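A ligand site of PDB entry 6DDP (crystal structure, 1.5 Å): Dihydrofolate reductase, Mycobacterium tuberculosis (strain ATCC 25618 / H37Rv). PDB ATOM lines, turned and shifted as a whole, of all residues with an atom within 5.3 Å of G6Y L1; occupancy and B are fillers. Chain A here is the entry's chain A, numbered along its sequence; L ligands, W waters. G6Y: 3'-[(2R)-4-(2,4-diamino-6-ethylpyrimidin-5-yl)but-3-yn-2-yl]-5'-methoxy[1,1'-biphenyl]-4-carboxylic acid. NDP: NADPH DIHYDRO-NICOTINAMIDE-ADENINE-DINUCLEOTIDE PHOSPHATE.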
ATOM      1  N   ILE A   5      26.770 -22.161  23.868  1.00  0.00           N
ATOM      2  CA  ILE A   5      26.105 -23.161  23.040  1.00  0.00           C
ATOM      3  C   ILE A   5      26.513 -22.931  21.589  1.00  0.00           C
ATOM      4  O   ILE A   5      26.479 -21.807  21.102  1.00  0.00           O
ATOM      5  CB  ILE A   5      24.570 -23.128  23.229  1.00  0.00           C
ATOM      6  CG1 ILE A   5      23.903 -24.190  22.352  1.00  0.00           C
ATOM      7  CG2 ILE A   5      24.004 -21.722  22.970  1.00  0.00           C
ATOM      8  CD1 ILE A   5      22.444 -24.463  22.746  1.00  0.00           C
ATOM      9  N   TRP A   6      26.947 -23.993  20.916  1.00  0.00           N
ATOM     10  CA  TRP A   6      27.318 -23.881  19.510  1.00  0.00           C
ATOM     11  C   TRP A   6      27.133 -25.197  18.791  1.00  0.00           C
ATOM     12  O   TRP A   6      27.030 -26.246  19.415  1.00  0.00           O
ATOM     13  CB  TRP A   6      28.772 -23.424  19.341  1.00  0.00           C
ATOM     14  CG  TRP A   6      29.858 -24.432  19.690  1.00  0.00           C
ATOM     15  CD1 TRP A   6      30.369 -25.410  18.877  1.00  0.00           C
ATOM     16  CD2 TRP A   6      30.600 -24.510  20.916  1.00  0.00           C
ATOM     17  NE1 TRP A   6      31.366 -26.097  19.537  1.00  0.00           N
ATOM     18  CE2 TRP A   6      31.526 -25.563  20.780  1.00  0.00           C
ATOM     19  CE3 TRP A   6      30.552 -23.785  22.122  1.00  0.00           C
ATOM     20  CZ2 TRP A   6      32.414 -25.922  21.812  1.00  0.00           C
ATOM     21  CZ3 TRP A   6      31.436 -24.149  23.146  1.00  0.00           C
ATOM     22  CH2 TRP A   6      32.362 -25.200  22.981  1.00  0.00           C
ATOM     23  N   ALA A   7      27.102 -25.118  17.457  1.00  0.00           N
ATOM     24  CA  ALA A   7      27.159 -26.289  16.606  1.00  0.00           C
ATOM     25  C   ALA A   7      28.417 -26.210  15.782  1.00  0.00           C
ATOM     26  O   ALA A   7      28.704 -25.174  15.183  1.00  0.00           O
ATOM     27  CB  ALA A   7      25.930 -26.357  15.705  1.00  0.00           C
ATOM     28  N   ILE A  20      26.475 -20.106   8.679  1.00  0.00           N
ATOM     29  CA  ILE A  20      26.739 -21.455   9.174  1.00  0.00           C
ATOM     30  C   ILE A  20      26.682 -22.402   7.994  1.00  0.00           C
ATOM     31  O   ILE A  20      25.668 -22.478   7.305  1.00  0.00           O
ATOM     32  CB  ILE A  20      25.715 -21.862  10.251  1.00  0.00           C
ATOM     33  CG1 ILE A  20      25.790 -20.898  11.436  1.00  0.00           C
ATOM     34  CG2 ILE A  20      25.955 -23.297  10.716  1.00  0.00           C
ATOM     35  CD1 ILE A  20      24.794 -21.213  12.551  1.00  0.00           C
ATOM     36  N   ASP A  27      19.053 -29.382  15.188  1.00  0.00           N
ATOM     37  CA  ASP A  27      19.911 -28.576  16.049  1.00  0.00           C
ATOM     38  C   ASP A  27      19.233 -27.286  16.454  1.00  0.00           C
ATOM     39  O   ASP A  27      19.373 -26.842  17.597  1.00  0.00           O
ATOM     40  CB  ASP A  27      21.226 -28.281  15.360  1.00  0.00           C
ATOM     41  CG  ASP A  27      22.079 -27.297  16.143  1.00  0.00           C
ATOM     42  OD1 ASP A  27      22.524 -27.638  17.247  1.00  0.00           O
ATOM     43  OD2 ASP A  27      22.292 -26.193  15.620  1.00  0.00           O
ATOM     44  N   GLN A  28      18.516 -26.676  15.516  1.00  0.00           N
ATOM     45  CA  GLN A  28      17.791 -25.435  15.807  1.00  0.00           C
ATOM     46  C   GLN A  28      16.773 -25.641  16.934  1.00  0.00           C
ATOM     47  O   GLN A  28      16.655 -24.795  17.822  1.00  0.00           O
ATOM     48  CB  GLN A  28      17.094 -24.902  14.551  1.00  0.00           C
ATOM     49  CG  GLN A  28      16.370 -23.588  14.741  1.00  0.00           C
ATOM     50  CD  GLN A  28      16.181 -22.834  13.442  1.00  0.00           C
ATOM     51  OE1 GLN A  28      17.135 -22.603  12.698  1.00  0.00           O
ATOM     52  NE2 GLN A  28      14.944 -22.467  13.148  1.00  0.00           N
ATOM     53  N   HIS A  30      16.957 -27.814  19.325  1.00  0.00           N
ATOM     54  CA  HIS A  30      17.756 -28.040  20.518  1.00  0.00           C
ATOM     55  C   HIS A  30      18.241 -26.722  21.095  1.00  0.00           C
ATOM     56  O   HIS A  30      18.186 -26.475  22.299  1.00  0.00           O
ATOM     57  CB  HIS A  30      18.933 -28.952  20.162  1.00  0.00           C
ATOM     58  CG  HIS A  30      20.027 -28.994  21.189  1.00  0.00           C
ATOM     59  ND1 HIS A  30      19.842 -29.521  22.454  1.00  0.00           N
ATOM     60  CD2 HIS A  30      21.307 -28.576  21.141  1.00  0.00           C
ATOM     61  CE1 HIS A  30      20.977 -29.429  23.127  1.00  0.00           C
ATOM     62  NE2 HIS A  30      21.876 -28.860  22.351  1.00  0.00           N
ATOM     63  N   PHE A  31      18.689 -25.865  20.187  1.00  0.00           N
ATOM     64  CA  PHE A  31      19.155 -24.530  20.538  1.00  0.00           C
ATOM     65  C   PHE A  31      18.027 -23.754  21.193  1.00  0.00           C
ATOM     66  O   PHE A  31      18.214 -23.085  22.217  1.00  0.00           O
ATOM     67  CB  PHE A  31      19.665 -23.827  19.275  1.00  0.00           C
ATOM     68  CG  PHE A  31      19.953 -22.373  19.459  1.00  0.00           C
ATOM     69  CD1 PHE A  31      21.185 -21.945  19.925  1.00  0.00           C
ATOM     70  CD2 PHE A  31      18.990 -21.429  19.155  1.00  0.00           C
ATOM     71  CE1 PHE A  31      21.440 -20.613  20.082  1.00  0.00           C
ATOM     72  CE2 PHE A  31      19.223 -20.097  19.312  1.00  0.00           C
ATOM     73  CZ  PHE A  31      20.469 -19.687  19.770  1.00  0.00           C
ATOM     74  N   ARG A  32      16.827 -23.880  20.628  1.00  0.00           N
ATOM     75  CA  ARG A  32      15.679 -23.158  21.129  1.00  0.00           C
ATOM     76  C   ARG A  32      15.319 -23.658  22.521  1.00  0.00           C
ATOM     77  O   ARG A  32      15.023 -22.871  23.422  1.00  0.00           O
ATOM     78  CB  ARG A  32      14.506 -23.335  20.165  1.00  0.00           C
ATOM     79  CG  ARG A  32      13.262 -22.559  20.527  1.00  0.00           C
ATOM     80  CD  ARG A  32      12.192 -22.728  19.453  1.00  0.00           C
ATOM     81  NE  ARG A  32      10.985 -21.983  19.789  1.00  0.00           N
ATOM     82  CZ  ARG A  32       9.958 -22.481  20.447  1.00  0.00           C
ATOM     83  NH1 ARG A  32       9.969 -23.753  20.839  1.00  0.00           N
ATOM     84  NH2 ARG A  32       8.897 -21.717  20.720  1.00  0.00           N
ATOM     85  N   MET A  36      15.527 -20.805  25.414  1.00  0.00           N
ATOM     86  CA  MET A  36      14.246 -20.136  25.586  1.00  0.00           C
ATOM     87  C   MET A  36      14.030 -19.599  26.999  1.00  0.00           C
ATOM     88  O   MET A  36      14.315 -20.275  27.983  1.00  0.00           O
ATOM     89  CB  MET A  36      13.106 -21.090  25.235  1.00  0.00           C
ATOM     90  CG  MET A  36      11.735 -20.420  25.180  1.00  0.00           C
ATOM     91  SD  MET A  36      11.661 -19.030  24.019  1.00  0.00           S
ATOM     92  CE  MET A  36      12.485 -19.704  22.584  1.00  0.00           C
ATOM     93  N   THR A  46      27.383 -11.956  14.572  1.00  0.00           N
ATOM     94  CA  THR A  46      26.390 -13.014  14.690  1.00  0.00           C
ATOM     95  C   THR A  46      24.994 -12.419  14.653  1.00  0.00           C
ATOM     96  O   THR A  46      24.085 -12.986  14.058  1.00  0.00           O
ATOM     97  CB  THR A  46      26.612 -13.821  15.968  1.00  0.00           C
ATOM     98  OG1 THR A  46      27.825 -14.582  15.825  1.00  0.00           O
ATOM     99  CG2 THR A  46      25.460 -14.767  16.223  1.00  0.00           C
ATOM    100  N   SER A  49      24.080 -11.868  11.129  1.00  0.00           N
ATOM    101  CA  SER A  49      23.829 -13.088  10.375  1.00  0.00           C
ATOM    102  C   SER A  49      22.405 -13.631  10.593  1.00  0.00           C
ATOM    103  O   SER A  49      21.942 -14.491   9.843  1.00  0.00           O
ATOM    104  CB  SER A  49      24.833 -14.175  10.738  1.00  0.00           C
ATOM    105  OG  SER A  49      24.508 -14.790  11.960  1.00  0.00           O
ATOM    106  N   LEU A  50      21.738 -13.151  11.635  1.00  0.00           N
ATOM    107  CA  LEU A  50      20.359 -13.564  11.907  1.00  0.00           C
ATOM    108  C   LEU A  50      19.431 -13.055  10.811  1.00  0.00           C
ATOM    109  O   LEU A  50      19.476 -11.877  10.458  1.00  0.00           O
ATOM    110  CB  LEU A  50      19.894 -13.059  13.270  1.00  0.00           C
ATOM    111  CG  LEU A  50      20.390 -13.747  14.544  1.00  0.00           C
ATOM    112  CD1 LEU A  50      19.986 -12.931  15.768  1.00  0.00           C
ATOM    113  CD2 LEU A  50      19.860 -15.174  14.654  1.00  0.00           C
ATOM    114  N   PRO A  51      18.598 -13.945  10.266  1.00  0.00           N
ATOM    115  CA  PRO A  51      17.545 -13.495   9.346  1.00  0.00           C
ATOM    116  C   PRO A  51      16.635 -12.497  10.036  1.00  0.00           C
ATOM    117  O   PRO A  51      16.437 -12.587  11.250  1.00  0.00           O
ATOM    118  CB  PRO A  51      16.805 -14.792   9.006  1.00  0.00           C
ATOM    119  CG  PRO A  51      17.800 -15.875   9.259  1.00  0.00           C
ATOM    120  CD  PRO A  51      18.614 -15.400  10.432  1.00  0.00           C
ATOM    121  N   VAL A  54      13.684 -13.382  12.399  1.00  0.00           N
ATOM    122  CA  VAL A  54      14.035 -14.019  13.663  1.00  0.00           C
ATOM    123  C   VAL A  54      15.021 -13.141  14.434  1.00  0.00           C
ATOM    124  O   VAL A  54      15.791 -13.598  15.290  1.00  0.00           O
ATOM    125  CB  VAL A  54      14.609 -15.429  13.386  1.00  0.00           C
ATOM    126  CG1 VAL A  54      16.065 -15.365  12.932  1.00  0.00           C
ATOM    127  CG2 VAL A  54      14.412 -16.297  14.601  1.00  0.00           C
ATOM    128  N   LEU A  57      15.801 -12.770  18.417  1.00  0.00           N
ATOM    129  CA  LEU A  57      15.268 -14.105  18.682  1.00  0.00           C
ATOM    130  C   LEU A  57      14.178 -13.971  19.730  1.00  0.00           C
ATOM    131  O   LEU A  57      14.418 -13.450  20.822  1.00  0.00           O
ATOM    132  CB  LEU A  57      16.375 -15.054  19.156  1.00  0.00           C
ATOM    133  CG  LEU A  57      17.306 -15.549  18.036  1.00  0.00           C
ATOM    134  CD1 LEU A  57      18.599 -16.140  18.596  1.00  0.00           C
ATOM    135  CD2 LEU A  57      16.625 -16.595  17.198  1.00  0.00           C
ATOM    136  N   ARG A  60      13.571 -14.507  24.163  1.00  0.00           N
ATOM    137  CA  ARG A  60      14.898 -14.430  24.774  1.00  0.00           C
ATOM    138  C   ARG A  60      15.320 -12.968  24.814  1.00  0.00           C
ATOM    139  O   ARG A  60      14.961 -12.202  23.918  1.00  0.00           O
ATOM    140  CB  ARG A  60      15.911 -15.257  23.974  1.00  0.00           C
ATOM    141  CG  ARG A  60      15.768 -16.757  24.187  1.00  0.00           C
ATOM    142  CD  ARG A  60      16.060 -17.574  22.932  1.00  0.00           C
ATOM    143  NE  ARG A  60      15.048 -17.422  21.898  1.00  0.00           N
ATOM    144  CZ  ARG A  60      14.970 -18.147  20.796  1.00  0.00           C
ATOM    145  NH1 ARG A  60      15.875 -19.096  20.535  1.00  0.00           N
ATOM    146  NH2 ARG A  60      13.996 -17.924  19.921  1.00  0.00           N
ATOM    147  N   VAL A  93      25.733 -17.783  25.826  1.00  0.00           N
ATOM    148  CA  VAL A  93      26.500 -17.151  24.758  1.00  0.00           C
ATOM    149  C   VAL A  93      26.332 -17.985  23.500  1.00  0.00           C
ATOM    150  O   VAL A  93      26.586 -19.180  23.503  1.00  0.00           O
ATOM    151  CB  VAL A  93      27.973 -17.019  25.138  1.00  0.00           C
ATOM    152  CG1 VAL A  93      28.757 -16.473  23.973  1.00  0.00           C
ATOM    153  CG2 VAL A  93      28.117 -16.106  26.336  1.00  0.00           C
ATOM    154  N   ILE A  94      25.842 -17.337  22.437  1.00  0.00           N
ATOM    155  CA  ILE A  94      25.388 -18.076  21.265  1.00  0.00           C
ATOM    156  C   ILE A  94      26.228 -17.778  20.019  1.00  0.00           C
ATOM    157  O   ILE A  94      25.858 -18.162  18.899  1.00  0.00           O
ATOM    158  CB  ILE A  94      23.889 -17.763  20.961  1.00  0.00           C
ATOM    159  CG1 ILE A  94      23.693 -16.312  20.515  1.00  0.00           C
ATOM    160  CG2 ILE A  94      23.042 -18.136  22.158  1.00  0.00           C
ATOM    161  CD1 ILE A  94      22.333 -16.042  19.865  1.00  0.00           C
ATOM    162  N   GLY A  95      27.368 -17.130  20.215  1.00  0.00           N
ATOM    163  CA  GLY A  95      28.305 -16.932  19.114  1.00  0.00           C
ATOM    164  C   GLY A  95      28.763 -15.502  18.961  1.00  0.00           C
ATOM    165  O   GLY A  95      28.245 -14.614  19.624  1.00  0.00           O
ATOM    166  N   TYR A 100      32.790 -16.445  21.761  1.00  0.00           N
ATOM    167  CA  TYR A 100      33.047 -17.694  22.505  1.00  0.00           C
ATOM    168  C   TYR A 100      34.392 -17.629  23.198  1.00  0.00           C
ATOM    169  O   TYR A 100      34.508 -18.031  24.352  1.00  0.00           O
ATOM    170  CB  TYR A 100      33.033 -18.921  21.599  1.00  0.00           C
ATOM    171  CG  TYR A 100      31.671 -19.311  21.057  1.00  0.00           C
ATOM    172  CD1 TYR A 100      30.540 -19.338  21.861  1.00  0.00           C
ATOM    173  CD2 TYR A 100      31.518 -19.647  19.726  1.00  0.00           C
ATOM    174  CE1 TYR A 100      29.294 -19.705  21.344  1.00  0.00           C
ATOM    175  CE2 TYR A 100      30.285 -20.003  19.206  1.00  0.00           C
ATOM    176  CZ  TYR A 100      29.181 -20.016  20.011  1.00  0.00           C
ATOM    177  OH  TYR A 100      27.983 -20.364  19.435  1.00  0.00           O
ATOM    178  N   GLU A 111      27.011 -26.447  25.690  1.00  0.00           N
ATOM    179  CA  GLU A 111      26.116 -27.367  25.009  1.00  0.00           C
ATOM    180  C   GLU A 111      26.544 -27.379  23.552  1.00  0.00           C
ATOM    181  O   GLU A 111      26.384 -26.385  22.834  1.00  0.00           O
ATOM    182  CB  GLU A 111      24.667 -26.938  25.203  1.00  0.00           C
ATOM    183  CG  GLU A 111      24.149 -27.089  26.631  1.00  0.00           C
ATOM    184  CD  GLU A 111      24.077 -28.542  27.101  1.00  0.00           C
ATOM    185  OE1 GLU A 111      23.901 -29.428  26.254  1.00  0.00           O
ATOM    186  OE2 GLU A 111      24.184 -28.783  28.319  1.00  0.00           O
ATOM    187  N   THR A 113      26.733 -29.156  19.695  1.00  0.00           N
ATOM    188  CA  THR A 113      26.307 -30.068  18.626  1.00  0.00           C
ATOM    189  C   THR A 113      27.459 -30.341  17.690  1.00  0.00           C
ATOM    190  O   THR A 113      28.062 -29.407  17.175  1.00  0.00           O
ATOM    191  CB  THR A 113      25.152 -29.478  17.828  1.00  0.00           C
ATOM    192  OG1 THR A 113      24.100 -29.136  18.719  1.00  0.00           O
ATOM    193  CG2 THR A 113      24.635 -30.475  16.782  1.00  0.00           C
HETATM  194  C4  G6Y L   1      22.927 -22.849  16.428  1.00  0.00           C
HETATM  195  C5  G6Y L   1      23.499 -21.755  17.070  1.00  0.00           C
HETATM  196  C6  G6Y L   1      24.155 -21.990  18.273  1.00  0.00           C
HETATM  197  N1  G6Y L   1      24.210 -23.220  18.801  1.00  0.00           N
HETATM  198  N3  G6Y L   1      23.012 -24.054  16.988  1.00  0.00           N
HETATM  199  CBE G6Y L   1      20.750 -22.968  15.382  1.00  0.00           C
HETATM  200  CBD G6Y L   1      22.251 -22.724  15.196  1.00  0.00           C
HETATM  201  C2  G6Y L   1      23.627 -24.245  18.168  1.00  0.00           C
HETATM  202  NAG G6Y L   1      23.682 -25.461  18.715  1.00  0.00           N
HETATM  203  NAH G6Y L   1      24.729 -20.955  18.903  1.00  0.00           N
HETATM  204  CAI G6Y L   1      23.410 -20.458  16.467  1.00  0.00           C
HETATM  205  CAJ G6Y L   1      23.286 -19.455  15.890  1.00  0.00           C
HETATM  206  CAK G6Y L   1      23.034 -18.247  15.076  1.00  0.00           C
HETATM  207  CBC G6Y L   1      22.829 -17.029  15.994  1.00  0.00           C
HETATM  208  CAL G6Y L   1      21.854 -18.444  14.301  1.00  0.00           C
HETATM  209  CAM G6Y L   1      20.611 -18.776  14.890  1.00  0.00           C
HETATM  210  CAQ G6Y L   1      21.902 -18.317  12.910  1.00  0.00           C
HETATM  211  CAP G6Y L   1      20.762 -18.505  12.146  1.00  0.00           C
HETATM  212  OAX G6Y L   1      20.855 -18.371  10.779  1.00  0.00           O
HETATM  213  CAY G6Y L   1      19.683 -18.845  10.102  1.00  0.00           C
HETATM  214  CAO G6Y L   1      19.546 -18.830  12.742  1.00  0.00           C
HETATM  215  CAN G6Y L   1      19.458 -18.995  14.117  1.00  0.00           C
HETATM  216  CAR G6Y L   1      18.224 -19.295  14.732  1.00  0.00           C
HETATM  217  CAS G6Y L   1      18.179 -19.850  16.005  1.00  0.00           C
HETATM  218  CAT G6Y L   1      16.962 -20.127  16.649  1.00  0.00           C
HETATM  219  CAU G6Y L   1      15.754 -19.845  16.010  1.00  0.00           C
HETATM  220  CAZ G6Y L   1      14.550 -20.119  16.657  1.00  0.00           C
HETATM  221  OBB G6Y L   1      14.519 -20.224  17.910  1.00  0.00           O
HETATM  222  OBA G6Y L   1      13.479 -20.225  16.014  1.00  0.00           O
HETATM  223  CAV G6Y L   1      15.786 -19.292  14.734  1.00  0.00           C
HETATM  224  CAW G6Y L   1      17.007 -19.010  14.097  1.00  0.00           C
HETATM  225  PA  NDP L   2      31.245 -12.519  16.390  1.00  0.00           P
HETATM  226  O1A NDP L   2      31.921 -13.104  17.544  1.00  0.00           O
HETATM  227  O2A NDP L   2      29.867 -12.993  16.035  1.00  0.00           O
HETATM  228  O5B NDP L   2      31.063 -10.902  16.592  1.00  0.00           O
HETATM  229  C5B NDP L   2      32.333 -10.290  16.554  1.00  0.00           C
HETATM  230  C4B NDP L   2      32.057  -8.816  16.952  1.00  0.00           C
HETATM  231  O4B NDP L   2      31.792  -8.735  18.327  1.00  0.00           O
HETATM  232  C3B NDP L   2      33.222  -7.848  16.659  1.00  0.00           C
HETATM  233  O3B NDP L   2      33.241  -7.465  15.325  1.00  0.00           O
HETATM  234  C2B NDP L   2      32.740  -6.654  17.540  1.00  0.00           C
HETATM  235  O2B NDP L   2      31.657  -6.060  17.060  1.00  0.00           O
HETATM  236  C1B NDP L   2      32.214  -7.441  18.792  1.00  0.00           C
HETATM  237  N9A NDP L   2      33.215  -7.654  19.812  1.00  0.00           N
HETATM  238  C8A NDP L   2      34.224  -8.642  19.842  1.00  0.00           C
HETATM  239  N7A NDP L   2      35.002  -8.573  20.945  1.00  0.00           N
HETATM  240  C5A NDP L   2      34.464  -7.490  21.650  1.00  0.00           C
HETATM  241  C6A NDP L   2      34.815  -6.916  22.873  1.00  0.00           C
HETATM  242  N6A NDP L   2      35.874  -7.427  23.597  1.00  0.00           N
HETATM  243  N1A NDP L   2      34.135  -5.854  23.373  1.00  0.00           N
HETATM  244  C2A NDP L   2      33.096  -5.397  22.594  1.00  0.00           C
HETATM  245  N3A NDP L   2      32.621  -5.841  21.416  1.00  0.00           N
HETATM  246  C4A NDP L   2      33.346  -6.911  20.952  1.00  0.00           C
HETATM  247  O3  NDP L   2      32.229 -12.549  15.003  1.00  0.00           O
HETATM  248  PN  NDP L   2      32.847 -13.944  14.463  1.00  0.00           P
HETATM  249  O1N NDP L   2      33.182 -13.672  13.052  1.00  0.00           O
HETATM  250  O2N NDP L   2      33.834 -14.605  15.389  1.00  0.00           O
HETATM  251  O5D NDP L   2      31.572 -15.146  14.386  1.00  0.00           O
HETATM  252  C5D NDP L   2      30.724 -14.958  13.294  1.00  0.00           C
HETATM  253  C4D NDP L   2      30.607 -16.315  12.552  1.00  0.00           C
HETATM  254  O4D NDP L   2      30.160 -17.350  13.472  1.00  0.00           O
HETATM  255  C3D NDP L   2      29.540 -16.257  11.413  1.00  0.00           C
HETATM  256  O3D NDP L   2      30.014 -17.032  10.338  1.00  0.00           O
HETATM  257  C2D NDP L   2      28.339 -16.940  12.067  1.00  0.00           C
HETATM  258  O2D NDP L   2      27.493 -17.550  11.131  1.00  0.00           O
HETATM  259  C1D NDP L   2      29.062 -18.045  12.881  1.00  0.00           C
HETATM  260  N1N NDP L   2      28.220 -18.575  13.971  1.00  0.00           N
HETATM  261  C2N NDP L   2      28.082 -19.947  14.138  1.00  0.00           C
HETATM  262  C3N NDP L   2      27.444 -20.449  15.223  1.00  0.00           C
HETATM  263  C7N NDP L   2      27.340 -21.882  15.375  1.00  0.00           C
HETATM  264  O7N NDP L   2      26.954 -22.411  16.413  1.00  0.00           O
HETATM  265  N7N NDP L   2      27.698 -22.674  14.299  1.00  0.00           N
HETATM  266  C4N NDP L   2      26.888 -19.596  16.287  1.00  0.00           C
HETATM  267  C5N NDP L   2      26.997 -18.167  15.982  1.00  0.00           C
HETATM  268  C6N NDP L   2      27.613 -17.703  14.897  1.00  0.00           C
HETATM  269  P2B NDP L   2      31.954  -4.483  16.231  1.00  0.00           P
HETATM  270  O1X NDP L   2      32.837  -5.040  15.146  1.00  0.00           O
HETATM  271  O2X NDP L   2      30.536  -4.060  15.835  1.00  0.00           O
HETATM  272  O3X NDP L   2      32.621  -3.729  17.347  1.00  0.00           O
HETATM  273  O   HOH W   1      24.240 -27.296  20.925  1.00  0.00           O
HETATM  274  O   HOH W   2      12.527 -20.329  13.681  1.00  0.00           O
HETATM  275  O   HOH W   3      24.940 -17.425  12.243  1.00  0.00           O
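OD2 of Asp 27 is in hydrogen-bond range of N3 of G6Y L1, 2.6 Å away.
O of Ile 5 is in hydrogen-bond range of NAH of G6Y L1.
The backbone carbonyl oxygen of Ile 94 sits at hydrogen-bond distance from a nitrogen (NAH) of G6Y L1, at 3.0 Å.
An oxygen (OBB) of G6Y L1 is in salt-bridge range of the guanidinium group of Arg 60 (3.1 Å).
A nitrogen (NAH) of G6Y L1 sits at hydrogen-bond distance from the side-chain hydroxyl of Tyr 100.
The backbone NH (N) of Thr 46 lies within hydrogen-bond range of an oxygen (O2A) of NDP L2, 3.1 Å away.
O2A of NDP L2 is in hydrogen-bond range of OG1 of Thr 46 (2.6 Å).
N of Ala 7 sits at hydrogen-bond distance from O7N of NDP L2 (2.9 Å).
The backbone carbonyl oxygen (O) of Ala 7 is in hydrogen-bond range of a nitrogen (N7N) of NDP L2 (2.8 Å).
The side-chain hydroxyl (OG1) of Thr 113 is in hydrogen-bond range of the side-chain carboxylate (OD1) of Asp 27 (2.6 Å).
O of Ile 5 sits at hydrogen-bond distance from OH of Tyr 100 (2.7 Å).
N of Ile 5 sits at hydrogen-bond distance from O of Val 93 (3.0 Å).
The side-chain hydroxyl of Tyr 100 sits at hydrogen-bond distance from the backbone carbonyl oxygen of Ile 94 (3.1 Å).
The backbone carbonyl oxygen (O) of Trp 6 is in hydrogen-bond range of the backbone NH (N) of Thr 113, 2.9 Å away.
The backbone carbonyl oxygen (O) of Glu 111 lies within hydrogen-bond range of the backbone NH (N) of Trp 6 (3.1 Å).
OH of Tyr 100 is in hydrogen-bond range of N of Gly 95 (3.4 Å).
O of Thr 46 is in hydrogen-bond range of OG of Ser 49, 2.8 Å away.
Residues that only touch G6Y L1: Trp 6, Ala 7, Ile 20, Gln 28, Phe 31, Arg 32, Thr 46, Leu 50, Pro 51, Val 54, Leu 57 and Thr 113.
Hydrophobic or aromatic side chains within 4 Å of G6Y L1: Ile 5, Ala 7, Ile 20, Phe 31, Leu 50, Pro 51, Val 54, Leu 57 and Ile 94.
Within 4 Å of G6Y L1: Ile 5, Trp 6, Ala 7, Ile 20, Asp 27, Gln 28, Phe 31, Arg 32, Thr 46, Leu 50, Pro 51, Val 54, Leu 57, Arg 60, Ile 94, Tyr 100 and Thr 113.
The nearest printed residue that does not touch G6Y L1 is Ser 49 (4.1 Å).
Water W2 lies within hydrogen-bond range of an oxygen (OBA) of G6Y L1 (2.5 Å) and the side-chain amide nitrogen of Gln 28 (3.3 Å).
Water W1 lies within hydrogen-bond range of OG1 of Thr 113 (2.9 Å), NAG of G6Y L1 (2.9 Å), O of Glu 111 (3.0 Å), NE2 of His 30 (3.2 Å) and O of Trp 6 (3.3 Å).
Water W3 lies within hydrogen-bond range of the side-chain hydroxyl (OG) of Ser 49 (2.7 Å) and an oxygen (O2D) of NDP L2 (2.8 Å).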
